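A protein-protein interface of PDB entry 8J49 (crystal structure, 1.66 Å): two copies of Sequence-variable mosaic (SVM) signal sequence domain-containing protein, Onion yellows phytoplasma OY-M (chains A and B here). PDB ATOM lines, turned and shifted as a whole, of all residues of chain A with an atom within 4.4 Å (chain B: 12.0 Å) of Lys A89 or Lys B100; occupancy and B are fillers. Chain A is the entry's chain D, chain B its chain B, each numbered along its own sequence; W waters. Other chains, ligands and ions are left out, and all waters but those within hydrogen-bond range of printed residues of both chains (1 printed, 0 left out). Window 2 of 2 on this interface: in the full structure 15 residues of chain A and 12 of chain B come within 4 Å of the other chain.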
ATOM      1  N   ARG A   3      30.216  15.870  11.234  1.00  0.00           N
ATOM      2  CA  ARG A   3      29.065  16.523  10.613  1.00  0.00           C
ATOM      3  C   ARG A   3      29.517  17.836   9.989  1.00  0.00           C
ATOM      4  O   ARG A   3      30.280  18.583  10.610  1.00  0.00           O
ATOM      5  CB  ARG A   3      27.946  16.770  11.641  1.00  0.00           C
ATOM      6  CG  ARG A   3      26.543  16.809  11.023  1.00  0.00           C
ATOM      7  CD  ARG A   3      25.775  15.589  11.538  1.00  0.00           C
ATOM      8  NE  ARG A   3      24.790  15.163  10.560  1.00  0.00           N
ATOM      9  CZ  ARG A   3      24.240  13.959  10.529  1.00  0.00           C
ATOM     10  NH1 ARG A   3      24.436  13.078  11.501  1.00  0.00           N
ATOM     11  NH2 ARG A   3      23.495  13.622   9.486  1.00  0.00           N
ATOM     12  N   ASP A   6      24.268  19.648   7.146  1.00  0.00           N
ATOM     13  CA  ASP A   6      23.363  18.522   7.010  1.00  0.00           C
ATOM     14  C   ASP A   6      24.042  17.270   6.460  1.00  0.00           C
ATOM     15  O   ASP A   6      23.357  16.274   6.199  1.00  0.00           O
ATOM     16  CB  ASP A   6      22.186  18.901   6.123  1.00  0.00           C
ATOM     17  CG  ASP A   6      21.289  19.942   6.761  1.00  0.00           C
ATOM     18  OD1 ASP A   6      21.356  20.116   7.998  1.00  0.00           O
ATOM     19  OD2 ASP A   6      20.523  20.586   6.017  1.00  0.00           O
ATOM     20  N   MET A   7      25.358  17.290   6.281  1.00  0.00           N
ATOM     21  CA  MET A   7      26.072  16.137   5.747  1.00  0.00           C
ATOM     22  C   MET A   7      26.685  15.339   6.883  1.00  0.00           C
ATOM     23  O   MET A   7      27.503  15.862   7.651  1.00  0.00           O
ATOM     24  CB  MET A   7      27.163  16.535   4.758  1.00  0.00           C
ATOM     25  CG  MET A   7      27.600  15.343   3.900  1.00  0.00           C
ATOM     26  SD  MET A   7      28.775  15.806   2.612  1.00  0.00           S
ATOM     27  CE  MET A   7      30.135  16.372   3.625  1.00  0.00           C
ATOM     28  N   ARG A   8      26.311  14.067   6.966  1.00  0.00           N
ATOM     29  CA  ARG A   8      26.968  13.154   7.888  1.00  0.00           C
ATOM     30  C   ARG A   8      28.245  12.648   7.232  1.00  0.00           C
ATOM     31  O   ARG A   8      28.230  12.257   6.065  1.00  0.00           O
ATOM     32  CB  ARG A   8      26.028  12.003   8.251  1.00  0.00           C
ATOM     33  CG  ARG A   8      26.561  11.058   9.329  1.00  0.00           C
ATOM     34  CD  ARG A   8      25.627   9.873   9.584  1.00  0.00           C
ATOM     35  NE  ARG A   8      25.321   9.094   8.391  1.00  0.00           N
ATOM     36  CZ  ARG A   8      25.224   7.769   8.360  1.00  0.00           C
ATOM     37  NH1 ARG A   8      25.371   7.036   9.452  1.00  0.00           N
ATOM     38  NH2 ARG A   8      24.981   7.163   7.199  1.00  0.00           N
ATOM     39  N   ASP A  65      26.926  10.555  -1.470  1.00  0.00           N
ATOM     40  CA  ASP A  65      25.783   9.738  -1.860  1.00  0.00           C
ATOM     41  C   ASP A  65      24.747  10.493  -2.681  1.00  0.00           C
ATOM     42  O   ASP A  65      23.739   9.899  -3.072  1.00  0.00           O
ATOM     43  CB  ASP A  65      25.128   9.090  -0.627  1.00  0.00           C
ATOM     44  CG  ASP A  65      24.365  10.068   0.250  1.00  0.00           C
ATOM     45  OD1 ASP A  65      24.418  11.305   0.044  1.00  0.00           O
ATOM     46  OD2 ASP A  65      23.689   9.573   1.173  1.00  0.00           O
ATOM     47  N   GLY A  87      25.114  19.246  -1.080  1.00  0.00           N
ATOM     48  CA  GLY A  87      23.803  18.678  -0.883  1.00  0.00           C
ATOM     49  C   GLY A  87      23.818  17.211  -0.517  1.00  0.00           C
ATOM     50  O   GLY A  87      22.796  16.691  -0.046  1.00  0.00           O
ATOM     51  N   ALA A  88      24.945  16.533  -0.721  1.00  0.00           N
ATOM     52  CA  ALA A  88      25.071  15.141  -0.324  1.00  0.00           C
ATOM     53  C   ALA A  88      24.680  14.977   1.136  1.00  0.00           C
ATOM     54  O   ALA A  88      25.112  15.746   2.009  1.00  0.00           O
ATOM     55  CB  ALA A  88      26.505  14.655  -0.561  1.00  0.00           C
ATOM     56  N   LYS A  89      23.831  13.982   1.391  1.00  0.00           N
ATOM     57  CA  LYS A  89      23.413  13.702   2.758  1.00  0.00           C
ATOM     58  C   LYS A  89      24.461  12.913   3.537  1.00  0.00           C
ATOM     59  O   LYS A  89      24.542  13.040   4.767  1.00  0.00           O
ATOM     60  CB  LYS A  89      22.071  12.974   2.735  1.00  0.00           C
ATOM     61  CG  LYS A  89      21.628  12.570   4.102  1.00  0.00           C
ATOM     62  CD  LYS A  89      20.882  13.679   4.783  1.00  0.00           C
ATOM     63  CE  LYS A  89      20.132  13.090   5.944  1.00  0.00           C
ATOM     64  NZ  LYS A  89      18.976  13.908   6.366  1.00  0.00           N
ATOM     65  N   ASN A  90      25.284  12.117   2.853  1.00  0.00           N
ATOM     66  CA  ASN A  90      26.335  11.358   3.514  1.00  0.00           C
ATOM     67  C   ASN A  90      27.600  11.394   2.673  1.00  0.00           C
ATOM     68  O   ASN A  90      27.544  11.254   1.449  1.00  0.00           O
ATOM     69  CB  ASN A  90      25.936   9.891   3.749  1.00  0.00           C
ATOM     70  CG  ASN A  90      24.654   9.750   4.549  1.00  0.00           C
ATOM     71  OD1 ASN A  90      24.670   9.806   5.775  1.00  0.00           O
ATOM     72  ND2 ASN A  90      23.537   9.570   3.851  1.00  0.00           N
ATOM     73  N   THR B  13      34.914  -2.936  10.039  1.00  0.00           N
ATOM     74  CA  THR B  13      33.554  -3.182   9.591  1.00  0.00           C
ATOM     75  C   THR B  13      33.556  -4.162   8.428  1.00  0.00           C
ATOM     76  O   THR B  13      34.406  -4.082   7.536  1.00  0.00           O
ATOM     77  CB  THR B  13      32.869  -1.859   9.193  1.00  0.00           C
ATOM     78  OG1 THR B  13      32.851  -0.978  10.323  1.00  0.00           O
ATOM     79  CG2 THR B  13      31.443  -2.091   8.751  1.00  0.00           C
ATOM     80  N   HIS B  57      23.573  -4.657  18.623  1.00  0.00           N
ATOM     81  CA  HIS B  57      23.000  -5.719  17.811  1.00  0.00           C
ATOM     82  C   HIS B  57      23.819  -6.025  16.561  1.00  0.00           C
ATOM     83  O   HIS B  57      23.591  -7.078  15.951  1.00  0.00           O
ATOM     84  CB  HIS B  57      21.557  -5.378  17.439  1.00  0.00           C
ATOM     85  CG  HIS B  57      21.437  -4.324  16.387  1.00  0.00           C
ATOM     86  ND1 HIS B  57      21.085  -4.617  15.087  1.00  0.00           N
ATOM     87  CD2 HIS B  57      21.631  -2.984  16.433  1.00  0.00           C
ATOM     88  CE1 HIS B  57      21.061  -3.500  14.378  1.00  0.00           C
ATOM     89  NE2 HIS B  57      21.391  -2.498  15.172  1.00  0.00           N
ATOM     90  N   ASN B  58      24.777  -5.168  16.182  1.00  0.00           N
ATOM     91  CA  ASN B  58      25.615  -5.407  15.011  1.00  0.00           C
ATOM     92  C   ASN B  58      27.068  -5.699  15.372  1.00  0.00           C
ATOM     93  O   ASN B  58      27.924  -5.734  14.486  1.00  0.00           O
ATOM     94  CB  ASN B  58      25.578  -4.213  14.059  1.00  0.00           C
ATOM     95  CG  ASN B  58      26.023  -2.923  14.721  1.00  0.00           C
ATOM     96  OD1 ASN B  58      25.867  -2.726  15.934  1.00  0.00           O
ATOM     97  ND2 ASN B  58      26.588  -2.023  13.917  1.00  0.00           N
ATOM     98  N   GLN B  96      29.315  -5.512  11.996  1.00  0.00           N
ATOM     99  CA  GLN B  96      28.589  -5.713  10.753  1.00  0.00           C
ATOM    100  C   GLN B  96      28.003  -4.378  10.297  1.00  0.00           C
ATOM    101  O   GLN B  96      27.370  -3.663  11.084  1.00  0.00           O
ATOM    102  CB  GLN B  96      27.495  -6.763  10.935  1.00  0.00           C
ATOM    103  CG  GLN B  96      26.537  -6.839   9.761  1.00  0.00           C
ATOM    104  CD  GLN B  96      25.871  -8.179   9.620  1.00  0.00           C
ATOM    105  OE1 GLN B  96      26.260  -9.160  10.262  1.00  0.00           O
ATOM    106  NE2 GLN B  96      24.832  -8.230   8.801  1.00  0.00           N
ATOM    107  N   TYR B  97      28.239  -4.031   9.034  1.00  0.00           N
ATOM    108  CA  TYR B  97      27.742  -2.755   8.533  1.00  0.00           C
ATOM    109  C   TYR B  97      26.222  -2.760   8.500  1.00  0.00           C
ATOM    110  O   TYR B  97      25.598  -3.748   8.104  1.00  0.00           O
ATOM    111  CB  TYR B  97      28.283  -2.466   7.132  1.00  0.00           C
ATOM    112  CG  TYR B  97      27.810  -1.129   6.589  1.00  0.00           C
ATOM    113  CD1 TYR B  97      28.289   0.064   7.117  1.00  0.00           C
ATOM    114  CD2 TYR B  97      26.857  -1.064   5.585  1.00  0.00           C
ATOM    115  CE1 TYR B  97      27.842   1.301   6.634  1.00  0.00           C
ATOM    116  CE2 TYR B  97      26.404   0.165   5.102  1.00  0.00           C
ATOM    117  CZ  TYR B  97      26.901   1.335   5.630  1.00  0.00           C
ATOM    118  OH  TYR B  97      26.457   2.555   5.155  1.00  0.00           O
ATOM    119  N   GLU B  98      25.619  -1.649   8.920  1.00  0.00           N
ATOM    120  CA  GLU B  98      24.208  -1.404   8.659  1.00  0.00           C
ATOM    121  C   GLU B  98      24.051  -0.024   8.031  1.00  0.00           C
ATOM    122  O   GLU B  98      24.772   0.916   8.383  1.00  0.00           O
ATOM    123  CB  GLU B  98      23.349  -1.492   9.929  1.00  0.00           C
ATOM    124  CG  GLU B  98      23.965  -0.940  11.204  1.00  0.00           C
ATOM    125  CD  GLU B  98      23.026  -1.138  12.392  1.00  0.00           C
ATOM    126  OE1 GLU B  98      21.951  -1.737  12.165  1.00  0.00           O
ATOM    127  OE2 GLU B  98      23.314  -0.665  13.517  1.00  0.00           O
ATOM    128  N   GLN B  99      23.116   0.093   7.097  1.00  0.00           N
ATOM    129  CA  GLN B  99      22.815   1.372   6.459  1.00  0.00           C
ATOM    130  C   GLN B  99      21.811   2.151   7.304  1.00  0.00           C
ATOM    131  O   GLN B  99      20.789   1.600   7.723  1.00  0.00           O
ATOM    132  CB  GLN B  99      22.277   1.140   5.047  1.00  0.00           C
ATOM    133  CG  GLN B  99      22.219   2.400   4.207  1.00  0.00           C
ATOM    134  CD  GLN B  99      23.613   2.858   3.813  1.00  0.00           C
ATOM    135  OE1 GLN B  99      24.109   3.869   4.318  1.00  0.00           O
ATOM    136  NE2 GLN B  99      24.275   2.085   2.956  1.00  0.00           N
ATOM    137  N   LYS B 100      22.113   3.430   7.558  1.00  0.00           N
ATOM    138  CA  LYS B 100      21.200   4.295   8.355  1.00  0.00           C
ATOM    139  C   LYS B 100      19.863   4.433   7.617  1.00  0.00           C
ATOM    140  O   LYS B 100      18.826   4.202   8.271  1.00  0.00           O
ATOM    141  CB  LYS B 100      21.836   5.670   8.585  1.00  0.00           C
ATOM    142  CG  LYS B 100      21.415   6.754   7.602  1.00  0.00           C
ATOM    143  CD  LYS B 100      21.435   8.147   8.198  1.00  0.00           C
ATOM    144  CE  LYS B 100      21.451   9.242   7.152  1.00  0.00           C
ATOM    145  NZ  LYS B 100      22.284  10.393   7.573  1.00  0.00           N
HETATM  146  O   HOH W   1      25.767   4.299   7.429  1.00  0.00           O
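Lys A89 touches just one residue of chain B: Lys B100.
Of the printed residues of chain A, Lys B100 touches Arg A3 (3.9 Å), Arg A8 (3.4 Å), Lys A89 (3.8 Å) and Asn A90 (3.0 Å).
Asp A6 touches none of the printed residues of chain B.
No residue of chain B comes within 4 Å of Met A7.
No residue of chain B comes within 4 Å of Asp A65.
Printed residues of chain B within 4 Å of Arg A3: Lys B100.
Tyr B97 touches none of the printed residues of chain A.
The nearest printed residue of chain A that does not touch Lys B100 is Asp A6 (6.1 Å).
No position is printed for both chains.
NH2 of Arg A3 touches NZ of Lys B100, at 3.9 Å.
Lys A89 touches Lys B100.
Water W1 bridges OH of Tyr B97 (2.9 Å) and NH2 of Arg A8 (3.0 Å).
Printed residues of chain B that touch a printed residue of chain A: Lys B100.
Among the printed residues, no Asp or Glu carboxylate lies within 4 Å of a Lys or Arg side-chain nitrogen of the other chain.
The side-chain amino group (NZ) of Lys B100 sits at hydrogen-bond distance from the side-chain amide oxygen (OD1) of Asn A90, 3.0 Å away.
NZ of Lys B100 sits close to NE of Arg A8.
The backbone NH (N) of Arg A8 lies within hydrogen-bond range of the backbone carbonyl oxygen (O) of Lys A89 (3.0 Å).
The guanidinium group of Arg A8 sits at hydrogen-bond distance from the side-chain amide oxygen of Asn A90 (2.8 Å).
OD1 of Asp A65 lies within hydrogen-bond range of N of Lys A89, at 3.1 Å.
OD2 of Asp A65 is in hydrogen-bond range of ND2 of Asn A90.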
